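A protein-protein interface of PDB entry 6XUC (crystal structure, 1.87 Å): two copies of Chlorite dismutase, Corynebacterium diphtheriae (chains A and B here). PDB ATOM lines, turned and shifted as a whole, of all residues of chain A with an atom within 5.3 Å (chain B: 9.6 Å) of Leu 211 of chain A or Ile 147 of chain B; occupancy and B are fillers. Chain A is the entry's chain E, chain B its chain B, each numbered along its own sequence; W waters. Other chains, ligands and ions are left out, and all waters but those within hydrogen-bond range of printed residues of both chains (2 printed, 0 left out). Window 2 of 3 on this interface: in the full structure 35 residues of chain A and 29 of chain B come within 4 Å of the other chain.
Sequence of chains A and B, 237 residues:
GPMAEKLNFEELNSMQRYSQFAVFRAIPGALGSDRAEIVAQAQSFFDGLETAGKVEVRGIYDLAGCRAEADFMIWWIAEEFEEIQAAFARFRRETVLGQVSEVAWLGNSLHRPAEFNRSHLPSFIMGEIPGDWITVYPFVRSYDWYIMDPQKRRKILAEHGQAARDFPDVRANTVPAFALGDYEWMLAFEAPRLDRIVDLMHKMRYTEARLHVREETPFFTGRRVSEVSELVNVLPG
OE1 of Glu 115 of chain B lies within hydrogen-bond range of OH of Tyr 206 of chain A (3.0 Å).
The side-chain carboxylate of Glu 115 of chain B lies within salt-bridge range of the guanidinium group of Arg 153 of chain B (2.8 Å).
The guanidinium group (NE) of Arg 214 of chain B lies within hydrogen-bond range of the backbone carbonyl oxygen (O) of Arg 141 of chain B (2.9 Å).
OH of Tyr 143 of chain B lies within hydrogen-bond range of NH1 of Arg 214 of chain B, 3.4 Å away.
The side-chain carboxylate (OD1) of Asp 144 of chain B is in hydrogen-bond range of a ring nitrogen (ND1) of His 212 of chain B, 2.9 Å away.
The backbone carbonyl oxygen (O) of Tyr 146 of chain B lies within hydrogen-bond range of the guanidinium group (NH1) of Arg 153 of chain B.
The backbone carbonyl oxygen of Met 148 of chain B lies within hydrogen-bond range of the guanidinium group of Arg 153 of chain B (3.0 Å).
Arg 205 of chain A touches Tyr 146 of chain B.
Arg 205 of chain A touches Ile 147 of chain B (O to N, 3.99 Å).
Tyr 206 of chain A touches Tyr 146 of chain B (CD2 to O, 3.0 Å).
Tyr 206 of chain A touches Ile 147 of chain B (C to CD1, 3.9 Å).
CE2 of Tyr 206 of chain A touches NH2 of Arg 153 of chain B, at 3.6 Å.
Thr 207 of chain A touches Ile 147 of chain B (O to CB, 3.6 Å).
NH2 of Arg 214 of chain B touches NH2 of Arg 210 of chain A, at 3.9 Å.
Leu 211 of chain A touches Asp 144 of chain B (CD2 to CA, 3.6 Å).
Ile 147 of chain B touches Leu 211 of chain A.
O of Val 213 of chain A touches CZ of Tyr 143 of chain B (3.4 Å).
Leu 211 of chain A touches just these residues of chain B: Asp 144 and Ile 147.
Of the printed residues of chain A, Ile 147 of chain B touches Arg 205, Tyr 206, Thr 207, Glu 208 and Leu 211.
No residue of chain B comes within 4 Å of Ala 209 of chain A.
Of the printed residues of chain B, Thr 207 of chain A touches Ile 147 (3.6 Å).
Of the printed residues of chain B, Tyr 206 of chain A touches Glu 115 (3.0 Å), Tyr 146 (3.0 Å), Ile 147 (3.9 Å) and Arg 153 (3.6 Å).
Printed residues of chain A within 4 Å of Tyr 146 of chain B: Arg 205 and Tyr 206.
Printed residues of chain B within 4 Å of Arg 205 of chain A: Tyr 146 (3.4 Å) and Ile 147 (3.99 Å).
Of the printed residues of chain A, Tyr 143 of chain B touches Arg 210 (3.4 Å) and Val 213 (3.4 Å).
Lys 152 of chain B touches none of the printed residues of chain A.
Arg 141 of chain B touches none of the printed residues of chain A.
The nearest residue of chain B that does not touch Leu 211 of chain A is Tyr 143 of chain B (4.2 Å).
The nearest printed residue of chain A that does not touch Ile 147 of chain B is Arg 210 of chain A (5.5 Å).
The nearest printed residue of chain B that does not touch Glu 208 of chain A is Tyr 143 of chain B (7.0 Å).
Of the 10 printed residues of chain A, 7 touch a printed residue of chain B.
Printed residues of chain A that touch a printed residue of chain B: Arg 205, Tyr 206, Thr 207, Glu 208, Arg 210, Leu 211 and Val 213.
Hydrophobic or aromatic side chains of chain A that line the printed part of chain B: Tyr 206, Leu 211 and Val 213.
Hydrophobic or aromatic side chains of chain B that line the printed part of chain A: Tyr 143, Tyr 146 and Ile 147.
2 positions are printed for both chains.
Water W1 lies within hydrogen-bond range of O of Tyr 143 of chain B, O of Arg 205 of chain A, N of Ile 147 of chain B and N of Tyr 146 of chain B.
Water W2 lies within hydrogen-bond range of NE of Arg 210 of chain A (2.8 Å) and O of Tyr 143 of chain B (3.0 Å).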
ATOM      1  N   SER A 142       2.191 -34.108 -27.703  1.00  0.00           N
ATOM      2  CA  SER A 142       2.563 -35.461 -27.364  1.00  0.00           C
ATOM      3  C   SER A 142       1.963 -36.433 -28.376  1.00  0.00           C
ATOM      4  O   SER A 142       0.973 -36.140 -29.064  1.00  0.00           O
ATOM      5  CB  SER A 142       2.086 -35.807 -25.956  1.00  0.00           C
ATOM      6  OG  SER A 142       0.720 -35.499 -25.834  1.00  0.00           O
ATOM      7  N   ARG A 205       0.763 -22.120 -18.237  1.00  0.00           N
ATOM      8  CA  ARG A 205       1.403 -23.337 -17.746  1.00  0.00           C
ATOM      9  C   ARG A 205       0.504 -24.103 -16.788  1.00  0.00           C
ATOM     10  O   ARG A 205       0.663 -25.323 -16.638  1.00  0.00           O
ATOM     11  CB  ARG A 205       2.707 -22.997 -17.024  1.00  0.00           C
ATOM     12  CG  ARG A 205       3.851 -22.587 -17.941  1.00  0.00           C
ATOM     13  CD  ARG A 205       4.145 -23.673 -18.999  1.00  0.00           C
ATOM     14  NE  ARG A 205       5.502 -23.627 -19.580  1.00  0.00           N
ATOM     15  CZ  ARG A 205       5.829 -23.083 -20.753  1.00  0.00           C
ATOM     16  NH1 ARG A 205       4.933 -22.496 -21.502  1.00  0.00           N
ATOM     17  NH2 ARG A 205       7.082 -23.145 -21.202  1.00  0.00           N
ATOM     18  N   TYR A 206      -0.440 -23.406 -16.170  1.00  0.00           N
ATOM     19  CA  TYR A 206      -1.330 -23.921 -15.144  1.00  0.00           C
ATOM     20  C   TYR A 206      -2.536 -24.558 -15.797  1.00  0.00           C
ATOM     21  O   TYR A 206      -3.681 -24.226 -15.497  1.00  0.00           O
ATOM     22  CB  TYR A 206      -1.735 -22.788 -14.205  1.00  0.00           C
ATOM     23  CG  TYR A 206      -0.595 -22.340 -13.343  1.00  0.00           C
ATOM     24  CD1 TYR A 206       0.389 -21.498 -13.851  1.00  0.00           C
ATOM     25  CD2 TYR A 206      -0.488 -22.754 -12.027  1.00  0.00           C
ATOM     26  CE1 TYR A 206       1.448 -21.075 -13.073  1.00  0.00           C
ATOM     27  CE2 TYR A 206       0.585 -22.338 -11.229  1.00  0.00           C
ATOM     28  CZ  TYR A 206       1.539 -21.496 -11.761  1.00  0.00           C
ATOM     29  OH  TYR A 206       2.598 -21.076 -10.996  1.00  0.00           O
ATOM     30  N   THR A 207      -2.254 -25.457 -16.743  1.00  0.00           N
ATOM     31  CA  THR A 207      -3.294 -26.090 -17.534  1.00  0.00           C
ATOM     32  C   THR A 207      -2.960 -27.556 -17.742  1.00  0.00           C
ATOM     33  O   THR A 207      -1.786 -27.925 -17.880  1.00  0.00           O
ATOM     34  CB  THR A 207      -3.450 -25.456 -18.922  1.00  0.00           C
ATOM     35  OG1 THR A 207      -2.176 -25.454 -19.572  1.00  0.00           O
ATOM     36  CG2 THR A 207      -3.994 -24.018 -18.820  1.00  0.00           C
ATOM     37  N   GLU A 208      -4.015 -28.383 -17.798  1.00  0.00           N
ATOM     38  CA  GLU A 208      -3.836 -29.805 -18.063  1.00  0.00           C
ATOM     39  C   GLU A 208      -3.223 -30.060 -19.439  1.00  0.00           C
ATOM     40  O   GLU A 208      -2.566 -31.087 -19.643  1.00  0.00           O
ATOM     41  CB  GLU A 208      -5.177 -30.550 -17.967  1.00  0.00           C
ATOM     42  CG  GLU A 208      -5.021 -32.047 -18.335  1.00  0.00           C
ATOM     43  CD  GLU A 208      -6.255 -32.866 -17.998  1.00  0.00           C
ATOM     44  OE1 GLU A 208      -7.259 -32.260 -17.588  1.00  0.00           O
ATOM     45  OE2 GLU A 208      -6.207 -34.103 -18.144  1.00  0.00           O
ATOM     46  N   ALA A 209      -3.444 -29.153 -20.394  1.00  0.00           N
ATOM     47  CA  ALA A 209      -2.910 -29.312 -21.743  1.00  0.00           C
ATOM     48  C   ALA A 209      -1.399 -29.454 -21.776  1.00  0.00           C
ATOM     49  O   ALA A 209      -0.844 -29.956 -22.769  1.00  0.00           O
ATOM     50  CB  ALA A 209      -3.294 -28.098 -22.585  1.00  0.00           C
ATOM     51  N   ARG A 210      -0.723 -28.947 -20.746  1.00  0.00           N
ATOM     52  CA  ARG A 210       0.722 -28.981 -20.700  1.00  0.00           C
ATOM     53  C   ARG A 210       1.226 -30.392 -20.537  1.00  0.00           C
ATOM     54  O   ARG A 210       2.419 -30.651 -20.736  1.00  0.00           O
ATOM     55  CB  ARG A 210       1.208 -28.116 -19.537  1.00  0.00           C
ATOM     56  CG  ARG A 210       0.924 -26.655 -19.699  1.00  0.00           C
ATOM     57  CD  ARG A 210       1.733 -26.067 -20.863  1.00  0.00           C
ATOM     58  NE  ARG A 210       3.151 -26.368 -20.813  1.00  0.00           N
ATOM     59  CZ  ARG A 210       4.013 -26.128 -21.803  1.00  0.00           C
ATOM     60  NH1 ARG A 210       3.611 -25.595 -22.948  1.00  0.00           N
ATOM     61  NH2 ARG A 210       5.307 -26.385 -21.633  1.00  0.00           N
ATOM     62  N   LEU A 211       0.364 -31.293 -20.094  1.00  0.00           N
ATOM     63  CA  LEU A 211       0.771 -32.681 -19.969  1.00  0.00           C
ATOM     64  C   LEU A 211       0.813 -33.376 -21.321  1.00  0.00           C
ATOM     65  O   LEU A 211       1.031 -34.580 -21.359  1.00  0.00           O
ATOM     66  CB  LEU A 211      -0.175 -33.424 -19.025  1.00  0.00           C
ATOM     67  CG  LEU A 211      -0.355 -32.835 -17.613  1.00  0.00           C
ATOM     68  CD1 LEU A 211      -1.499 -33.644 -16.903  1.00  0.00           C
ATOM     69  CD2 LEU A 211       0.959 -32.812 -16.800  1.00  0.00           C
ATOM     70  N   HIS A 212       0.572 -32.659 -22.425  1.00  0.00           N
ATOM     71  CA  HIS A 212       0.502 -33.284 -23.752  1.00  0.00           C
ATOM     72  C   HIS A 212       1.278 -32.416 -24.750  1.00  0.00           C
ATOM     73  O   HIS A 212       0.809 -32.077 -25.828  1.00  0.00           O
ATOM     74  CB  HIS A 212      -0.960 -33.517 -24.163  1.00  0.00           C
ATOM     75  CG  HIS A 212      -1.745 -34.290 -23.141  1.00  0.00           C
ATOM     76  ND1 HIS A 212      -1.659 -35.661 -23.017  1.00  0.00           N
ATOM     77  CD2 HIS A 212      -2.588 -33.878 -22.163  1.00  0.00           C
ATOM     78  CE1 HIS A 212      -2.415 -36.061 -22.008  1.00  0.00           C
ATOM     79  NE2 HIS A 212      -2.979 -34.996 -21.464  1.00  0.00           N
ATOM     80  N   VAL A 213       2.542 -32.165 -24.408  1.00  0.00           N
ATOM     81  CA  VAL A 213       3.453 -31.328 -25.185  1.00  0.00           C
ATOM     82  C   VAL A 213       4.749 -32.089 -25.392  1.00  0.00           C
ATOM     83  O   VAL A 213       5.220 -32.754 -24.468  1.00  0.00           O
ATOM     84  CB  VAL A 213       3.727 -29.997 -24.439  1.00  0.00           C
ATOM     85  CG1 VAL A 213       4.740 -29.114 -25.174  1.00  0.00           C
ATOM     86  CG2 VAL A 213       2.422 -29.286 -24.160  1.00  0.00           C
ATOM     87  N   GLU B 115       5.197 -17.317  -6.468  1.00  0.00           N
ATOM     88  CA  GLU B 115       3.857 -17.882  -6.399  1.00  0.00           C
ATOM     89  C   GLU B 115       3.364 -17.917  -4.966  1.00  0.00           C
ATOM     90  O   GLU B 115       2.233 -17.512  -4.676  1.00  0.00           O
ATOM     91  CB  GLU B 115       3.853 -19.300  -7.001  1.00  0.00           C
ATOM     92  CG  GLU B 115       2.441 -19.883  -7.135  1.00  0.00           C
ATOM     93  CD  GLU B 115       2.366 -21.263  -7.777  1.00  0.00           C
ATOM     94  OE1 GLU B 115       3.396 -21.821  -8.246  1.00  0.00           O
ATOM     95  OE2 GLU B 115       1.242 -21.789  -7.787  1.00  0.00           O
ATOM     96  N   ARG B 141      11.121 -26.269 -16.055  1.00  0.00           N
ATOM     97  CA  ARG B 141      10.496 -27.239 -15.175  1.00  0.00           C
ATOM     98  C   ARG B 141       9.877 -28.400 -15.951  1.00  0.00           C
ATOM     99  O   ARG B 141       9.559 -28.293 -17.135  1.00  0.00           O
ATOM    100  CB  ARG B 141       9.416 -26.545 -14.356  1.00  0.00           C
ATOM    101  CG  ARG B 141       9.963 -25.735 -13.201  1.00  0.00           C
ATOM    102  CD  ARG B 141      10.264 -26.649 -12.006  1.00  0.00           C
ATOM    103  NE  ARG B 141      10.870 -25.872 -10.934  1.00  0.00           N
ATOM    104  CZ  ARG B 141      11.812 -26.310 -10.117  1.00  0.00           C
ATOM    105  NH1 ARG B 141      12.274 -27.547 -10.235  1.00  0.00           N
ATOM    106  NH2 ARG B 141      12.304 -25.491  -9.197  1.00  0.00           N
ATOM    107  N   SER B 142       9.625 -29.496 -15.234  1.00  0.00           N
ATOM    108  CA  SER B 142       8.856 -30.591 -15.797  1.00  0.00           C
ATOM    109  C   SER B 142       7.489 -30.109 -16.294  1.00  0.00           C
ATOM    110  O   SER B 142       6.969 -29.086 -15.859  1.00  0.00           O
ATOM    111  CB  SER B 142       8.673 -31.697 -14.756  1.00  0.00           C
ATOM    112  OG  SER B 142       8.128 -31.183 -13.562  1.00  0.00           O
ATOM    113  N   TYR B 143       6.920 -30.864 -17.242  1.00  0.00           N
ATOM    114  CA  TYR B 143       5.627 -30.470 -17.795  1.00  0.00           C
ATOM    115  C   TYR B 143       4.550 -30.434 -16.722  1.00  0.00           C
ATOM    116  O   TYR B 143       3.626 -29.623 -16.814  1.00  0.00           O
ATOM    117  CB  TYR B 143       5.198 -31.408 -18.915  1.00  0.00           C
ATOM    118  CG  TYR B 143       5.960 -31.224 -20.207  1.00  0.00           C
ATOM    119  CD1 TYR B 143       5.887 -30.034 -20.915  1.00  0.00           C
ATOM    120  CD2 TYR B 143       6.782 -32.232 -20.687  1.00  0.00           C
ATOM    121  CE1 TYR B 143       6.570 -29.869 -22.076  1.00  0.00           C
ATOM    122  CE2 TYR B 143       7.500 -32.069 -21.846  1.00  0.00           C
ATOM    123  CZ  TYR B 143       7.366 -30.898 -22.550  1.00  0.00           C
ATOM    124  OH  TYR B 143       8.034 -30.744 -23.724  1.00  0.00           O
ATOM    125  N   ASP B 144       4.650 -31.290 -15.698  1.00  0.00           N
ATOM    126  CA  ASP B 144       3.583 -31.412 -14.694  1.00  0.00           C
ATOM    127  C   ASP B 144       3.671 -30.373 -13.572  1.00  0.00           C
ATOM    128  O   ASP B 144       2.810 -30.350 -12.684  1.00  0.00           O
ATOM    129  CB  ASP B 144       3.617 -32.824 -14.094  1.00  0.00           C
ATOM    130  CG  ASP B 144       4.808 -33.052 -13.183  1.00  0.00           C
ATOM    131  OD1 ASP B 144       5.664 -32.156 -13.035  1.00  0.00           O
ATOM    132  OD2 ASP B 144       4.878 -34.138 -12.572  1.00  0.00           O
ATOM    133  N   TRP B 145       4.699 -29.533 -13.579  1.00  0.00           N
ATOM    134  CA  TRP B 145       5.039 -28.765 -12.382  1.00  0.00           C
ATOM    135  C   TRP B 145       3.976 -27.747 -12.017  1.00  0.00           C
ATOM    136  O   TRP B 145       3.670 -27.567 -10.834  1.00  0.00           O
ATOM    137  CB  TRP B 145       6.367 -28.063 -12.593  1.00  0.00           C
ATOM    138  CG  TRP B 145       6.812 -27.089 -11.524  1.00  0.00           C
ATOM    139  CD1 TRP B 145       6.916 -25.745 -11.659  1.00  0.00           C
ATOM    140  CD2 TRP B 145       7.242 -27.394 -10.201  1.00  0.00           C
ATOM    141  NE1 TRP B 145       7.397 -25.180 -10.504  1.00  0.00           N
ATOM    142  CE2 TRP B 145       7.611 -26.173  -9.591  1.00  0.00           C
ATOM    143  CE3 TRP B 145       7.358 -28.576  -9.467  1.00  0.00           C
ATOM    144  CZ2 TRP B 145       8.093 -26.101  -8.291  1.00  0.00           C
ATOM    145  CZ3 TRP B 145       7.854 -28.504  -8.184  1.00  0.00           C
ATOM    146  CH2 TRP B 145       8.191 -27.272  -7.598  1.00  0.00           C
ATOM    147  N   TYR B 146       3.447 -27.032 -12.997  1.00  0.00           N
ATOM    148  CA  TYR B 146       2.531 -25.931 -12.716  1.00  0.00           C
ATOM    149  C   TYR B 146       1.078 -26.365 -12.561  1.00  0.00           C
ATOM    150  O   TYR B 146       0.317 -25.690 -11.856  1.00  0.00           O
ATOM    151  CB  TYR B 146       2.569 -24.912 -13.860  1.00  0.00           C
ATOM    152  CG  TYR B 146       3.998 -24.437 -14.150  1.00  0.00           C
ATOM    153  CD1 TYR B 146       4.539 -23.388 -13.433  1.00  0.00           C
ATOM    154  CD2 TYR B 146       4.797 -25.056 -15.099  1.00  0.00           C
ATOM    155  CE1 TYR B 146       5.832 -22.951 -13.652  1.00  0.00           C
ATOM    156  CE2 TYR B 146       6.097 -24.601 -15.343  1.00  0.00           C
ATOM    157  CZ  TYR B 146       6.587 -23.543 -14.621  1.00  0.00           C
ATOM    158  OH  TYR B 146       7.868 -23.092 -14.825  1.00  0.00           O
ATOM    159  N   ILE B 147       0.665 -27.441 -13.254  1.00  0.00           N
ATOM    160  CA  ILE B 147      -0.705 -27.955 -13.101  1.00  0.00           C
ATOM    161  C   ILE B 147      -0.820 -28.852 -11.884  1.00  0.00           C
ATOM    162  O   ILE B 147      -1.932 -29.099 -11.416  1.00  0.00           O
ATOM    163  CB  ILE B 147      -1.167 -28.697 -14.368  1.00  0.00           C
ATOM    164  CG1 ILE B 147      -2.676 -29.001 -14.314  1.00  0.00           C
ATOM    165  CG2 ILE B 147      -0.337 -29.960 -14.592  1.00  0.00           C
ATOM    166  CD1 ILE B 147      -3.595 -27.773 -13.903  1.00  0.00           C
ATOM    167  N   MET B 148       0.295 -29.259 -11.288  1.00  0.00           N
ATOM    168  CA  MET B 148       0.239 -30.047 -10.057  1.00  0.00           C
ATOM    169  C   MET B 148      -0.555 -29.297  -8.982  1.00  0.00           C
ATOM    170  O   MET B 148      -0.669 -28.073  -8.998  1.00  0.00           O
ATOM    171  CB  MET B 148       1.675 -30.361  -9.599  1.00  0.00           C
ATOM    172  CG  MET B 148       1.900 -30.553  -8.114  1.00  0.00           C
ATOM    173  SD  MET B 148       3.663 -30.501  -7.665  1.00  0.00           S
ATOM    174  CE  MET B 148       4.329 -31.382  -9.063  1.00  0.00           C
ATOM    175  N   ASP B 149      -1.119 -30.058  -8.035  1.00  0.00           N
ATOM    176  CA  ASP B 149      -1.882 -29.459  -6.944  1.00  0.00           C
ATOM    177  C   ASP B 149      -1.049 -28.385  -6.253  1.00  0.00           C
ATOM    178  O   ASP B 149       0.088 -28.666  -5.819  1.00  0.00           O
ATOM    179  CB  ASP B 149      -2.292 -30.540  -5.937  1.00  0.00           C
ATOM    180  CG  ASP B 149      -3.202 -30.029  -4.827  1.00  0.00           C
ATOM    181  OD1 ASP B 149      -3.316 -28.808  -4.587  1.00  0.00           O
ATOM    182  OD2 ASP B 149      -3.807 -30.885  -4.159  1.00  0.00           O
ATOM    183  N   PRO B 150      -1.567 -27.154  -6.122  1.00  0.00           N
ATOM    184  CA  PRO B 150      -0.750 -26.077  -5.534  1.00  0.00           C
ATOM    185  C   PRO B 150      -0.183 -26.436  -4.173  1.00  0.00           C
ATOM    186  O   PRO B 150       0.977 -26.114  -3.872  1.00  0.00           O
ATOM    187  CB  PRO B 150      -1.737 -24.898  -5.450  1.00  0.00           C
ATOM    188  CG  PRO B 150      -2.745 -25.192  -6.526  1.00  0.00           C
ATOM    189  CD  PRO B 150      -2.921 -26.686  -6.488  1.00  0.00           C
ATOM    190  N   GLN B 151      -0.974 -27.118  -3.350  1.00  0.00           N
ATOM    191  CA  GLN B 151      -0.509 -27.546  -2.030  1.00  0.00           C
ATOM    192  C   GLN B 151       0.731 -28.423  -2.159  1.00  0.00           C
ATOM    193  O   GLN B 151       1.651 -28.349  -1.336  1.00  0.00           O
ATOM    194  CB  GLN B 151      -1.658 -28.276  -1.308  1.00  0.00           C
ATOM    195  CG  GLN B 151      -1.309 -28.977   0.016  1.00  0.00           C
ATOM    196  CD  GLN B 151      -2.390 -29.977   0.500  1.00  0.00           C
ATOM    197  OE1 GLN B 151      -3.216 -30.464  -0.281  1.00  0.00           O
ATOM    198  NE2 GLN B 151      -2.368 -30.286   1.795  1.00  0.00           N
ATOM    199  N   LYS B 152       0.792 -29.250  -3.194  1.00  0.00           N
ATOM    200  CA  LYS B 152       1.940 -30.128  -3.310  1.00  0.00           C
ATOM    201  C   LYS B 152       3.131 -29.337  -3.823  1.00  0.00           C
ATOM    202  O   LYS B 152       4.249 -29.504  -3.328  1.00  0.00           O
ATOM    203  CB  LYS B 152       1.609 -31.326  -4.198  1.00  0.00           C
ATOM    204  CG  LYS B 152       2.713 -32.358  -4.157  1.00  0.00           C
ATOM    205  CD  LYS B 152       2.413 -33.670  -4.863  1.00  0.00           C
ATOM    206  CE  LYS B 152       3.607 -34.068  -5.746  1.00  0.00           C
ATOM    207  NZ  LYS B 152       3.692 -35.505  -6.116  1.00  0.00           N
ATOM    208  N   ARG B 153       2.891 -28.413  -4.751  1.00  0.00           N
ATOM    209  CA  ARG B 153       3.985 -27.581  -5.237  1.00  0.00           C
ATOM    210  C   ARG B 153       4.491 -26.653  -4.135  1.00  0.00           C
ATOM    211  O   ARG B 153       5.680 -26.365  -4.069  1.00  0.00           O
ATOM    212  CB  ARG B 153       3.554 -26.766  -6.469  1.00  0.00           C
ATOM    213  CG  ARG B 153       4.697 -25.969  -7.075  1.00  0.00           C
ATOM    214  CD  ARG B 153       4.297 -25.258  -8.403  1.00  0.00           C
ATOM    215  NE  ARG B 153       3.010 -24.596  -8.239  1.00  0.00           N
ATOM    216  CZ  ARG B 153       1.837 -25.130  -8.546  1.00  0.00           C
ATOM    217  NH1 ARG B 153       1.766 -26.357  -9.067  1.00  0.00           N
ATOM    218  NH2 ARG B 153       0.731 -24.442  -8.310  1.00  0.00           N
ATOM    219  N   HIS B 212      11.322 -32.654 -10.824  1.00  0.00           N
ATOM    220  CA  HIS B 212      10.418 -31.820 -11.632  1.00  0.00           C
ATOM    221  C   HIS B 212      11.244 -30.825 -12.446  1.00  0.00           C
ATOM    222  O   HIS B 212      10.952 -29.629 -12.530  1.00  0.00           O
ATOM    223  CB  HIS B 212       9.379 -31.154 -10.729  1.00  0.00           C
ATOM    224  CG  HIS B 212       8.444 -32.131 -10.083  1.00  0.00           C
ATOM    225  ND1 HIS B 212       7.397 -32.709 -10.769  1.00  0.00           N
ATOM    226  CD2 HIS B 212       8.459 -32.716  -8.859  1.00  0.00           C
ATOM    227  CE1 HIS B 212       6.767 -33.563  -9.977  1.00  0.00           C
ATOM    228  NE2 HIS B 212       7.400 -33.603  -8.817  1.00  0.00           N
ATOM    229  N   ARG B 214      13.331 -30.268 -16.277  1.00  0.00           N
ATOM    230  CA  ARG B 214      13.510 -30.701 -17.657  1.00  0.00           C
ATOM    231  C   ARG B 214      14.777 -30.175 -18.320  1.00  0.00           C
ATOM    232  O   ARG B 214      15.321 -30.881 -19.177  1.00  0.00           O
ATOM    233  CB  ARG B 214      12.325 -30.261 -18.540  1.00  0.00           C
ATOM    234  CG  ARG B 214      11.286 -31.289 -18.792  1.00  0.00           C
ATOM    235  CD  ARG B 214      10.385 -30.892 -19.952  1.00  0.00           C
ATOM    236  NE  ARG B 214       9.629 -29.662 -19.742  1.00  0.00           N
ATOM    237  CZ  ARG B 214       9.488 -28.723 -20.671  1.00  0.00           C
ATOM    238  NH1 ARG B 214      10.089 -28.876 -21.841  1.00  0.00           N
ATOM    239  NH2 ARG B 214       8.796 -27.638 -20.420  1.00  0.00           N
HETATM  240  O   HOH W   1       2.065 -27.584 -15.788  1.00  0.00           O
HETATM  241  O   HOH W   2       4.385 -27.274 -18.441  1.00  0.00           O
